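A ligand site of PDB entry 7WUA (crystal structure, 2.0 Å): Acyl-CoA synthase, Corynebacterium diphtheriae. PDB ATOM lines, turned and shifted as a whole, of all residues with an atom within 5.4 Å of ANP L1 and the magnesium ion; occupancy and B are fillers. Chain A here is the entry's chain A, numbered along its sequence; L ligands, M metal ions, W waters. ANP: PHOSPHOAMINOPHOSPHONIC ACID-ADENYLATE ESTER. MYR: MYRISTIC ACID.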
ATOM      1  N   THR A 200       1.316 -32.491 -26.832  1.00  0.00           N
ATOM      2  CA  THR A 200       2.307 -31.457 -27.053  1.00  0.00           C
ATOM      3  C   THR A 200       3.701 -32.076 -27.189  1.00  0.00           C
ATOM      4  O   THR A 200       3.897 -33.276 -26.972  1.00  0.00           O
ATOM      5  CB  THR A 200       2.282 -30.449 -25.900  1.00  0.00           C
ATOM      6  OG1 THR A 200       2.337 -31.149 -24.662  1.00  0.00           O
ATOM      7  CG2 THR A 200       1.015 -29.591 -25.961  1.00  0.00           C
ATOM      8  N   SER A 201       4.662 -31.235 -27.549  1.00  0.00           N
ATOM      9  CA  SER A 201       6.036 -31.663 -27.765  1.00  0.00           C
ATOM     10  C   SER A 201       6.991 -30.777 -26.967  1.00  0.00           C
ATOM     11  O   SER A 201       6.604 -29.771 -26.378  1.00  0.00           O
ATOM     12  CB  SER A 201       6.393 -31.625 -29.268  1.00  0.00           C
ATOM     13  OG  SER A 201       6.687 -30.300 -29.688  1.00  0.00           O
ATOM     14  N   GLY A 202       8.261 -31.184 -26.973  1.00  0.00           N
ATOM     15  CA  GLY A 202       9.301 -30.468 -26.265  1.00  0.00           C
ATOM     16  C   GLY A 202       9.586 -30.971 -24.876  1.00  0.00           C
ATOM     17  O   GLY A 202      10.601 -30.579 -24.279  1.00  0.00           O
ATOM     18  N   SER A 203       8.715 -31.795 -24.315  1.00  0.00           N
ATOM     19  CA  SER A 203       8.958 -32.398 -23.017  1.00  0.00           C
ATOM     20  C   SER A 203       9.623 -33.757 -23.202  1.00  0.00           C
ATOM     21  O   SER A 203       9.379 -34.464 -24.191  1.00  0.00           O
ATOM     22  CB  SER A 203       7.646 -32.548 -22.236  1.00  0.00           C
ATOM     23  OG  SER A 203       7.676 -33.670 -21.357  1.00  0.00           O
ATOM     24  N   ASP A 245      -0.331 -27.172 -31.365  1.00  0.00           N
ATOM     25  CA  ASP A 245      -1.485 -26.423 -30.895  1.00  0.00           C
ATOM     26  C   ASP A 245      -1.694 -25.137 -31.695  1.00  0.00           C
ATOM     27  O   ASP A 245      -2.784 -24.867 -32.205  1.00  0.00           O
ATOM     28  CB  ASP A 245      -1.283 -26.118 -29.414  1.00  0.00           C
ATOM     29  CG  ASP A 245      -2.451 -25.407 -28.783  1.00  0.00           C
ATOM     30  OD1 ASP A 245      -3.586 -25.893 -28.948  1.00  0.00           O
ATOM     31  OD2 ASP A 245      -2.222 -24.361 -28.116  1.00  0.00           O
ATOM     32  N   ILE A 321       2.998 -12.953 -32.256  1.00  0.00           N
ATOM     33  CA  ILE A 321       4.232 -13.618 -31.890  1.00  0.00           C
ATOM     34  C   ILE A 321       4.012 -14.323 -30.563  1.00  0.00           C
ATOM     35  O   ILE A 321       3.519 -13.711 -29.610  1.00  0.00           O
ATOM     36  CB  ILE A 321       5.419 -12.645 -31.791  1.00  0.00           C
ATOM     37  CG1 ILE A 321       5.426 -11.681 -32.984  1.00  0.00           C
ATOM     38  CG2 ILE A 321       6.732 -13.410 -31.705  1.00  0.00           C
ATOM     39  CD1 ILE A 321       5.808 -10.261 -32.610  1.00  0.00           C
ATOM     40  N   GLY A 322       4.385 -15.599 -30.496  1.00  0.00           N
ATOM     41  CA  GLY A 322       4.192 -16.367 -29.283  1.00  0.00           C
ATOM     42  C   GLY A 322       4.673 -17.797 -29.444  1.00  0.00           C
ATOM     43  O   GLY A 322       5.263 -18.163 -30.466  1.00  0.00           O
ATOM     44  N   SER A 323       4.418 -18.591 -28.402  1.00  0.00           N
ATOM     45  CA  SER A 323       4.815 -19.985 -28.192  1.00  0.00           C
ATOM     46  C   SER A 323       6.162 -20.082 -27.481  1.00  0.00           C
ATOM     47  O   SER A 323       6.543 -21.166 -27.049  1.00  0.00           O
ATOM     48  CB  SER A 323       4.855 -20.833 -29.478  1.00  0.00           C
ATOM     49  OG  SER A 323       6.042 -20.630 -30.228  1.00  0.00           O
ATOM     50  N   GLU A 324       6.877 -18.971 -27.345  1.00  0.00           N
ATOM     51  CA  GLU A 324       8.111 -18.905 -26.556  1.00  0.00           C
ATOM     52  C   GLU A 324       8.314 -17.450 -26.148  1.00  0.00           C
ATOM     53  O   GLU A 324       7.639 -16.563 -26.672  1.00  0.00           O
ATOM     54  CB  GLU A 324       9.315 -19.434 -27.348  1.00  0.00           C
ATOM     55  CG  GLU A 324       9.634 -18.578 -28.596  1.00  0.00           C
ATOM     56  CD  GLU A 324      10.841 -19.064 -29.381  1.00  0.00           C
ATOM     57  OE1 GLU A 324      11.647 -19.871 -28.851  1.00  0.00           O
ATOM     58  OE2 GLU A 324      10.990 -18.647 -30.555  1.00  0.00           O
ATOM     59  N   PRO A 325       9.212 -17.186 -25.212  1.00  0.00           N
ATOM     60  CA  PRO A 325       9.410 -15.803 -24.772  1.00  0.00           C
ATOM     61  C   PRO A 325       9.720 -14.907 -25.969  1.00  0.00           C
ATOM     62  O   PRO A 325      10.592 -15.209 -26.791  1.00  0.00           O
ATOM     63  CB  PRO A 325      10.596 -15.904 -23.812  1.00  0.00           C
ATOM     64  CG  PRO A 325      10.502 -17.293 -23.260  1.00  0.00           C
ATOM     65  CD  PRO A 325      10.041 -18.131 -24.442  1.00  0.00           C
ATOM     66  N   VAL A 326       8.972 -13.819 -26.082  1.00  0.00           N
ATOM     67  CA  VAL A 326       9.182 -12.835 -27.129  1.00  0.00           C
ATOM     68  C   VAL A 326      10.205 -11.818 -26.613  1.00  0.00           C
ATOM     69  O   VAL A 326      10.054 -11.295 -25.507  1.00  0.00           O
ATOM     70  CB  VAL A 326       7.862 -12.158 -27.519  1.00  0.00           C
ATOM     71  CG1 VAL A 326       8.070 -11.103 -28.604  1.00  0.00           C
ATOM     72  CG2 VAL A 326       6.826 -13.237 -27.965  1.00  0.00           C
ATOM     73  N   SER A 351       1.700 -12.518 -27.886  1.00  0.00           N
ATOM     74  CA  SER A 351       0.540 -13.170 -27.289  1.00  0.00           C
ATOM     75  C   SER A 351       0.959 -14.464 -26.609  1.00  0.00           C
ATOM     76  O   SER A 351       2.008 -15.033 -26.920  1.00  0.00           O
ATOM     77  CB  SER A 351      -0.549 -13.468 -28.338  1.00  0.00           C
ATOM     78  OG  SER A 351      -0.907 -12.301 -29.040  1.00  0.00           O
ATOM     79  N   TYR A 352       0.109 -14.950 -25.703  1.00  0.00           N
ATOM     80  CA  TYR A 352       0.458 -16.050 -24.830  1.00  0.00           C
ATOM     81  C   TYR A 352      -0.687 -17.049 -24.743  1.00  0.00           C
ATOM     82  O   TYR A 352      -1.859 -16.657 -24.680  1.00  0.00           O
ATOM     83  CB  TYR A 352       0.805 -15.537 -23.424  1.00  0.00           C
ATOM     84  CG  TYR A 352       0.761 -16.629 -22.387  1.00  0.00           C
ATOM     85  CD1 TYR A 352       1.818 -17.506 -22.231  1.00  0.00           C
ATOM     86  CD2 TYR A 352      -0.361 -16.785 -21.564  1.00  0.00           C
ATOM     87  CE1 TYR A 352       1.772 -18.516 -21.281  1.00  0.00           C
ATOM     88  CE2 TYR A 352      -0.406 -17.795 -20.614  1.00  0.00           C
ATOM     89  CZ  TYR A 352       0.659 -18.656 -20.471  1.00  0.00           C
ATOM     90  OH  TYR A 352       0.606 -19.645 -19.530  1.00  0.00           O
ATOM     91  N   GLY A 353      -0.345 -18.326 -24.716  1.00  0.00           N
ATOM     92  CA  GLY A 353      -1.336 -19.376 -24.570  1.00  0.00           C
ATOM     93  C   GLY A 353      -0.678 -20.735 -24.407  1.00  0.00           C
ATOM     94  O   GLY A 353       0.547 -20.858 -24.307  1.00  0.00           O
ATOM     95  N   LEU A 354      -1.522 -21.753 -24.359  1.00  0.00           N
ATOM     96  CA  LEU A 354      -1.028 -23.110 -24.191  1.00  0.00           C
ATOM     97  C   LEU A 354      -2.184 -24.054 -24.483  1.00  0.00           C
ATOM     98  O   LEU A 354      -3.353 -23.684 -24.359  1.00  0.00           O
ATOM     99  CB  LEU A 354      -0.462 -23.341 -22.781  1.00  0.00           C
ATOM    100  CG  LEU A 354      -1.402 -23.312 -21.565  1.00  0.00           C
ATOM    101  CD1 LEU A 354      -0.662 -23.778 -20.311  1.00  0.00           C
ATOM    102  CD2 LEU A 354      -2.030 -21.919 -21.336  1.00  0.00           C
ATOM    103  N   ALA A 355      -1.832 -25.285 -24.862  1.00  0.00           N
ATOM    104  CA  ALA A 355      -2.846 -26.259 -25.270  1.00  0.00           C
ATOM    105  C   ALA A 355      -3.886 -26.478 -24.180  1.00  0.00           C
ATOM    106  O   ALA A 355      -5.054 -26.700 -24.483  1.00  0.00           O
ATOM    107  CB  ALA A 355      -2.161 -27.581 -25.653  1.00  0.00           C
ATOM    108  N   GLU A 356      -3.479 -26.399 -22.907  1.00  0.00           N
ATOM    109  CA  GLU A 356      -4.423 -26.642 -21.817  1.00  0.00           C
ATOM    110  C   GLU A 356      -5.556 -25.623 -21.794  1.00  0.00           C
ATOM    111  O   GLU A 356      -6.586 -25.880 -21.174  1.00  0.00           O
ATOM    112  CB  GLU A 356      -3.683 -26.616 -20.477  1.00  0.00           C
ATOM    113  CG  GLU A 356      -2.848 -27.851 -20.198  1.00  0.00           C
ATOM    114  CD  GLU A 356      -1.492 -27.822 -20.890  1.00  0.00           C
ATOM    115  OE1 GLU A 356      -1.206 -26.849 -21.623  1.00  0.00           O
ATOM    116  OE2 GLU A 356      -0.725 -28.791 -20.709  1.00  0.00           O
ATOM    117  N   VAL A 400       2.523  -9.375 -23.206  1.00  0.00           N
ATOM    118  CA  VAL A 400       1.681 -10.228 -24.047  1.00  0.00           C
ATOM    119  C   VAL A 400       0.200  -9.897 -23.878  1.00  0.00           C
ATOM    120  O   VAL A 400      -0.655 -10.716 -24.185  1.00  0.00           O
ATOM    121  CB  VAL A 400       1.957 -11.721 -23.790  1.00  0.00           C
ATOM    122  CG1 VAL A 400       3.339 -12.096 -24.301  1.00  0.00           C
ATOM    123  CG2 VAL A 400       1.814 -12.073 -22.309  1.00  0.00           C
ATOM    124  N   THR A 476      -0.899 -23.146 -15.014  1.00  0.00           N
ATOM    125  CA  THR A 476      -0.196 -23.242 -16.300  1.00  0.00           C
ATOM    126  C   THR A 476       1.219 -23.803 -16.176  1.00  0.00           C
ATOM    127  O   THR A 476       1.778 -24.256 -17.181  1.00  0.00           O
ATOM    128  CB  THR A 476      -0.083 -21.867 -16.964  1.00  0.00           C
ATOM    129  OG1 THR A 476       0.665 -20.992 -16.107  1.00  0.00           O
ATOM    130  CG2 THR A 476      -1.451 -21.274 -17.225  1.00  0.00           C
ATOM    131  N   ASP A 478       3.577 -21.759 -15.757  1.00  0.00           N
ATOM    132  CA  ASP A 478       4.319 -20.632 -16.272  1.00  0.00           C
ATOM    133  C   ASP A 478       4.380 -19.536 -15.215  1.00  0.00           C
ATOM    134  O   ASP A 478       3.380 -19.261 -14.549  1.00  0.00           O
ATOM    135  CB  ASP A 478       3.672 -20.060 -17.540  1.00  0.00           C
ATOM    136  CG  ASP A 478       3.718 -21.019 -18.695  1.00  0.00           C
ATOM    137  OD1 ASP A 478       4.778 -21.656 -18.917  1.00  0.00           O
ATOM    138  OD2 ASP A 478       2.677 -21.134 -19.378  1.00  0.00           O
ATOM    139  N   ILE A 489       5.551 -12.684 -19.284  1.00  0.00           N
ATOM    140  CA  ILE A 489       5.974 -14.047 -18.985  1.00  0.00           C
ATOM    141  C   ILE A 489       7.460 -14.026 -18.639  1.00  0.00           C
ATOM    142  O   ILE A 489       8.280 -13.541 -19.433  1.00  0.00           O
ATOM    143  CB  ILE A 489       5.723 -14.990 -20.181  1.00  0.00           C
ATOM    144  CG1 ILE A 489       4.285 -14.843 -20.699  1.00  0.00           C
ATOM    145  CG2 ILE A 489       6.028 -16.430 -19.780  1.00  0.00           C
ATOM    146  CD1 ILE A 489       3.197 -15.316 -19.733  1.00  0.00           C
ATOM    147  N   ARG A 492       9.180 -20.727 -17.425  1.00  0.00           N
ATOM    148  CA  ARG A 492       8.492 -21.915 -16.949  1.00  0.00           C
ATOM    149  C   ARG A 492       8.901 -22.212 -15.503  1.00  0.00           C
ATOM    150  O   ARG A 492      10.084 -22.274 -15.192  1.00  0.00           O
ATOM    151  CB  ARG A 492       8.812 -23.125 -17.832  1.00  0.00           C
ATOM    152  CG  ARG A 492       8.393 -22.974 -19.310  1.00  0.00           C
ATOM    153  CD  ARG A 492       8.853 -24.188 -20.124  1.00  0.00           C
ATOM    154  NE  ARG A 492       8.611 -24.046 -21.559  1.00  0.00           N
ATOM    155  CZ  ARG A 492       7.554 -24.526 -22.202  1.00  0.00           C
ATOM    156  NH1 ARG A 492       6.602 -25.164 -21.527  1.00  0.00           N
ATOM    157  NH2 ARG A 492       7.433 -24.343 -23.507  1.00  0.00           N
ATOM    158  N   ARG A 594      14.277 -28.109 -22.896  1.00  0.00           N
ATOM    159  CA  ARG A 594      14.256 -29.286 -22.028  1.00  0.00           C
ATOM    160  C   ARG A 594      14.853 -30.491 -22.741  1.00  0.00           C
ATOM    161  O   ARG A 594      15.546 -31.319 -22.122  1.00  0.00           O
ATOM    162  CB  ARG A 594      12.830 -29.565 -21.559  1.00  0.00           C
ATOM    163  CG  ARG A 594      12.304 -28.493 -20.617  1.00  0.00           C
ATOM    164  CD  ARG A 594      10.778 -28.470 -20.568  1.00  0.00           C
ATOM    165  NE  ARG A 594      10.194 -28.029 -21.831  1.00  0.00           N
ATOM    166  CZ  ARG A 594       8.970 -28.353 -22.239  1.00  0.00           C
ATOM    167  NH1 ARG A 594       8.189 -29.116 -21.483  1.00  0.00           N
ATOM    168  NH2 ARG A 594       8.518 -27.913 -23.410  1.00  0.00           N
HETATM  169  PG  ANP L   1       4.664 -29.747 -22.898  1.00  0.00           P
HETATM  170  O1G ANP L   1       4.539 -31.088 -23.383  1.00  0.00           O
HETATM  171  O2G ANP L   1       5.713 -29.699 -21.830  1.00  0.00           O
HETATM  172  O3G ANP L   1       3.379 -29.314 -22.323  1.00  0.00           O
HETATM  173  PB  ANP L   1       4.600 -27.062 -24.326  1.00  0.00           P
HETATM  174  O1B ANP L   1       4.289 -26.605 -22.931  1.00  0.00           O
HETATM  175  O2B ANP L   1       5.693 -26.262 -24.911  1.00  0.00           O
HETATM  176  N3B ANP L   1       5.143 -28.685 -24.238  1.00  0.00           N
HETATM  177  PA  ANP L   1       2.328 -25.792 -25.757  1.00  0.00           P
HETATM  178  O1A ANP L   1       2.130 -25.759 -27.274  1.00  0.00           O
HETATM  179  O2A ANP L   1       1.015 -25.917 -25.101  1.00  0.00           O
HETATM  180  O3A ANP L   1       3.268 -27.043 -25.305  1.00  0.00           O
HETATM  181  O5' ANP L   1       3.093 -24.397 -25.332  1.00  0.00           O
HETATM  182  C5' ANP L   1       2.544 -23.563 -24.298  1.00  0.00           C
HETATM  183  C4' ANP L   1       3.736 -22.998 -23.563  1.00  0.00           C
HETATM  184  O4' ANP L   1       4.491 -22.333 -24.397  1.00  0.00           O
HETATM  185  C3' ANP L   1       3.253 -22.049 -22.329  1.00  0.00           C
HETATM  186  O3' ANP L   1       3.005 -22.769 -21.275  1.00  0.00           O
HETATM  187  C2' ANP L   1       4.540 -21.194 -22.284  1.00  0.00           C
HETATM  188  O2' ANP L   1       5.517 -21.982 -21.446  1.00  0.00           O
HETATM  189  C1' ANP L   1       5.088 -21.069 -23.528  1.00  0.00           C
HETATM  190  N9  ANP L   1       4.683 -19.901 -24.144  1.00  0.00           N
HETATM  191  C8  ANP L   1       3.674 -19.749 -24.994  1.00  0.00           C
HETATM  192  N7  ANP L   1       3.578 -18.475 -25.369  1.00  0.00           N
HETATM  193  C5  ANP L   1       4.558 -17.795 -24.726  1.00  0.00           C
HETATM  194  C6  ANP L   1       5.006 -16.438 -24.667  1.00  0.00           C
HETATM  195  N6  ANP L   1       4.341 -15.444 -25.434  1.00  0.00           N
HETATM  196  N1  ANP L   1       6.044 -16.107 -23.903  1.00  0.00           N
HETATM  197  C2  ANP L   1       6.687 -17.037 -23.165  1.00  0.00           C
HETATM  198  N3  ANP L   1       6.302 -18.305 -23.201  1.00  0.00           N
HETATM  199  C4  ANP L   1       5.248 -18.705 -23.968  1.00  0.00           C
HETATM  200  C1  MYR L   2       1.254 -22.250 -27.639  1.00  0.00           C
HETATM  201  O1  MYR L   2       0.882 -23.443 -27.454  1.00  0.00           O
HETATM  202  O2  MYR L   2       2.481 -21.959 -27.583  1.00  0.00           O
HETATM  203  C2  MYR L   2       0.221 -21.173 -27.957  1.00  0.00           C
HETATM  204  C3  MYR L   2       0.760 -19.754 -27.812  1.00  0.00           C
HETATM  205  C4  MYR L   2       0.534 -18.939 -29.082  1.00  0.00           C
HETATM  206  C5  MYR L   2      -0.590 -17.900 -29.042  1.00  0.00           C
HETATM  207  C6  MYR L   2      -1.116 -17.682 -30.481  1.00  0.00           C
HETATM  208  C7  MYR L   2      -2.238 -16.660 -30.611  1.00  0.00           C
HETATM  209  C8  MYR L   2      -3.072 -16.868 -31.877  1.00  0.00           C
HETATM  210  C9  MYR L   2      -4.396 -16.092 -31.830  1.00  0.00           C
HETATM  211  C10 MYR L   2      -4.452 -14.904 -32.810  1.00  0.00           C
HETATM  212  C11 MYR L   2      -5.268 -15.215 -34.067  1.00  0.00           C
HETATM  213  C12 MYR L   2      -5.509 -14.020 -34.987  1.00  0.00           C
HETATM  214  C13 MYR L   2      -5.143 -14.376 -36.429  1.00  0.00           C
HETATM  215  C14 MYR L   2      -6.271 -14.212 -37.451  1.00  0.00           C
HETATM  216 MG    MG M   1       3.116 -27.423 -21.155  1.00  0.00          MG
HETATM  217  O   HOH W   1       7.892 -19.963 -21.446  1.00  0.00           O
HETATM  218  O   HOH W   2       5.439 -23.807 -27.042  1.00  0.00           O
HETATM  219  O   HOH W   3       6.744 -13.437 -24.167  1.00  0.00           O
HETATM  220  O   HOH W   4       6.964 -26.488 -27.211  1.00  0.00           O
HETATM  221  O   HOH W   5       1.772 -28.059 -19.775  1.00  0.00           O
HETATM  222  O   HOH W   6       4.812 -27.789 -20.134  1.00  0.00           O
HETATM  223  O   HOH W   7       1.232 -26.919 -22.591  1.00  0.00           O
HETATM  224  O   HOH W   8       2.934 -25.613 -20.856  1.00  0.00           O
HETATM  225  O   HOH W   9       1.435 -27.804 -29.279  1.00  0.00           O
HETATM  226  O   HOH W  10       1.006 -30.162 -22.475  1.00  0.00           O
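OD2 of Asp 478 sits at hydrogen-bond distance from O3' of ANP L1 (2.5 Å).
The side-chain hydroxyl (OG1) of Thr 200 sits at hydrogen-bond distance from an oxygen (O1G) of ANP L1 (2.5 Å).
The guanidinium group (NH1) of Arg 594 is in salt-bridge range of an oxygen (O2G) of ANP L1 (2.6 Å).
A nitrogen (N6) of ANP L1 is in hydrogen-bond range of the backbone carbonyl oxygen (O) of Ser 351 (2.8 Å).
N3B of ANP L1 lies within hydrogen-bond range of O of Ser 201 (2.8 Å).
The backbone NH (N) of Ala 355 lies within hydrogen-bond range of an oxygen (O2A) of ANP L1 (2.9 Å).
The guanidinium group (NH2) of Arg 492 is in salt-bridge range of an oxygen (O2B) of ANP L1 (2.9 Å).
The backbone NH (N) of Ser 323 sits at hydrogen-bond distance from a nitrogen (N7) of ANP L1, 3.1 Å away.
O1A of ANP L1 lies close to O1 of MYR L2, 2.6 Å away.
OH of Tyr 352 lies within hydrogen-bond range of OD2 of Asp 478, 2.6 Å away.
The side-chain hydroxyl (OG1) of Thr 476 is in hydrogen-bond range of the backbone NH (N) of Asp 478 (3.0 Å).
O of Gly 202 lies close to NH2 of Arg 594.
N of Ser 351 is in hydrogen-bond range of O of Ile 321, 2.8 Å away.
The side-chain carboxylate of Asp 245 is in hydrogen-bond range of the backbone NH of Ala 355 (3.4 Å).
A nitrogen (N1) of ANP L1 sits close to the backbone carbonyl oxygen (O) of Glu 324 (3.2 Å).
Ser 203 touches ANP L1 (CB to O2G, 3.5 Å).
CA of Gly 322 touches N6 of ANP L1 (3.96 Å).
N of Pro 325 touches C2 of ANP L1 (3.3 Å).
Tyr 352 touches ANP L1.
Gly 353 touches ANP L1 (O to C5', 3.4 Å).
Leu 354 touches ANP L1 (CB to C5', 3.4 Å).
CG1 of Val 400 touches N6 of ANP L1 (3.7 Å).
Ile 489 touches ANP L1.
Hydrophobic or aromatic side chains within 4 Å of ANP L1: Pro 325, Tyr 352, Leu 354, Ala 355, Val 400 and Ile 489.
Of the 23 residues printed, 17 come within 4 Å of ANP L1.
No residue comes within 4 Å of the magnesium ion.
The nearest printed residue that does not touch the magnesium ion is Glu 356 (4.1 Å).
The magnesium ion is bound by water W8 (1.8 Å), water W6 (2.0 Å), water W5 (2.0 Å), an oxygen (O3G) of ANP L1 (2.2 Å), an oxygen (O1B) of ANP L1 (2.3 Å) and water W7 (2.4 Å).
The magnesium ion has six donor atoms within binding distance.
Water W7 bridges the side-chain carboxylate (OE1) of Glu 356 (2.6 Å) and an oxygen (O2A) of ANP L1 (2.7 Å).
Water W6 bridges an oxygen (O2G) of ANP L1 and the guanidinium group (NH1) of Arg 492.
Water W10 lies within hydrogen-bond range of the side-chain hydroxyl (OG1) of Thr 200 (2.7 Å) and the side-chain carboxylate (OE2) of Glu 356 (2.8 Å).
Water W4 bridges O2B of ANP L1 (2.6 Å) and O of Ser 201 (3.4 Å).
Water W9 lies within hydrogen-bond range of N of Asp 245 and O1A of ANP L1.
Water W2 lies within hydrogen-bond range of O of Ser 323 (2.9 Å) and O5' of ANP L1 (3.0 Å).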
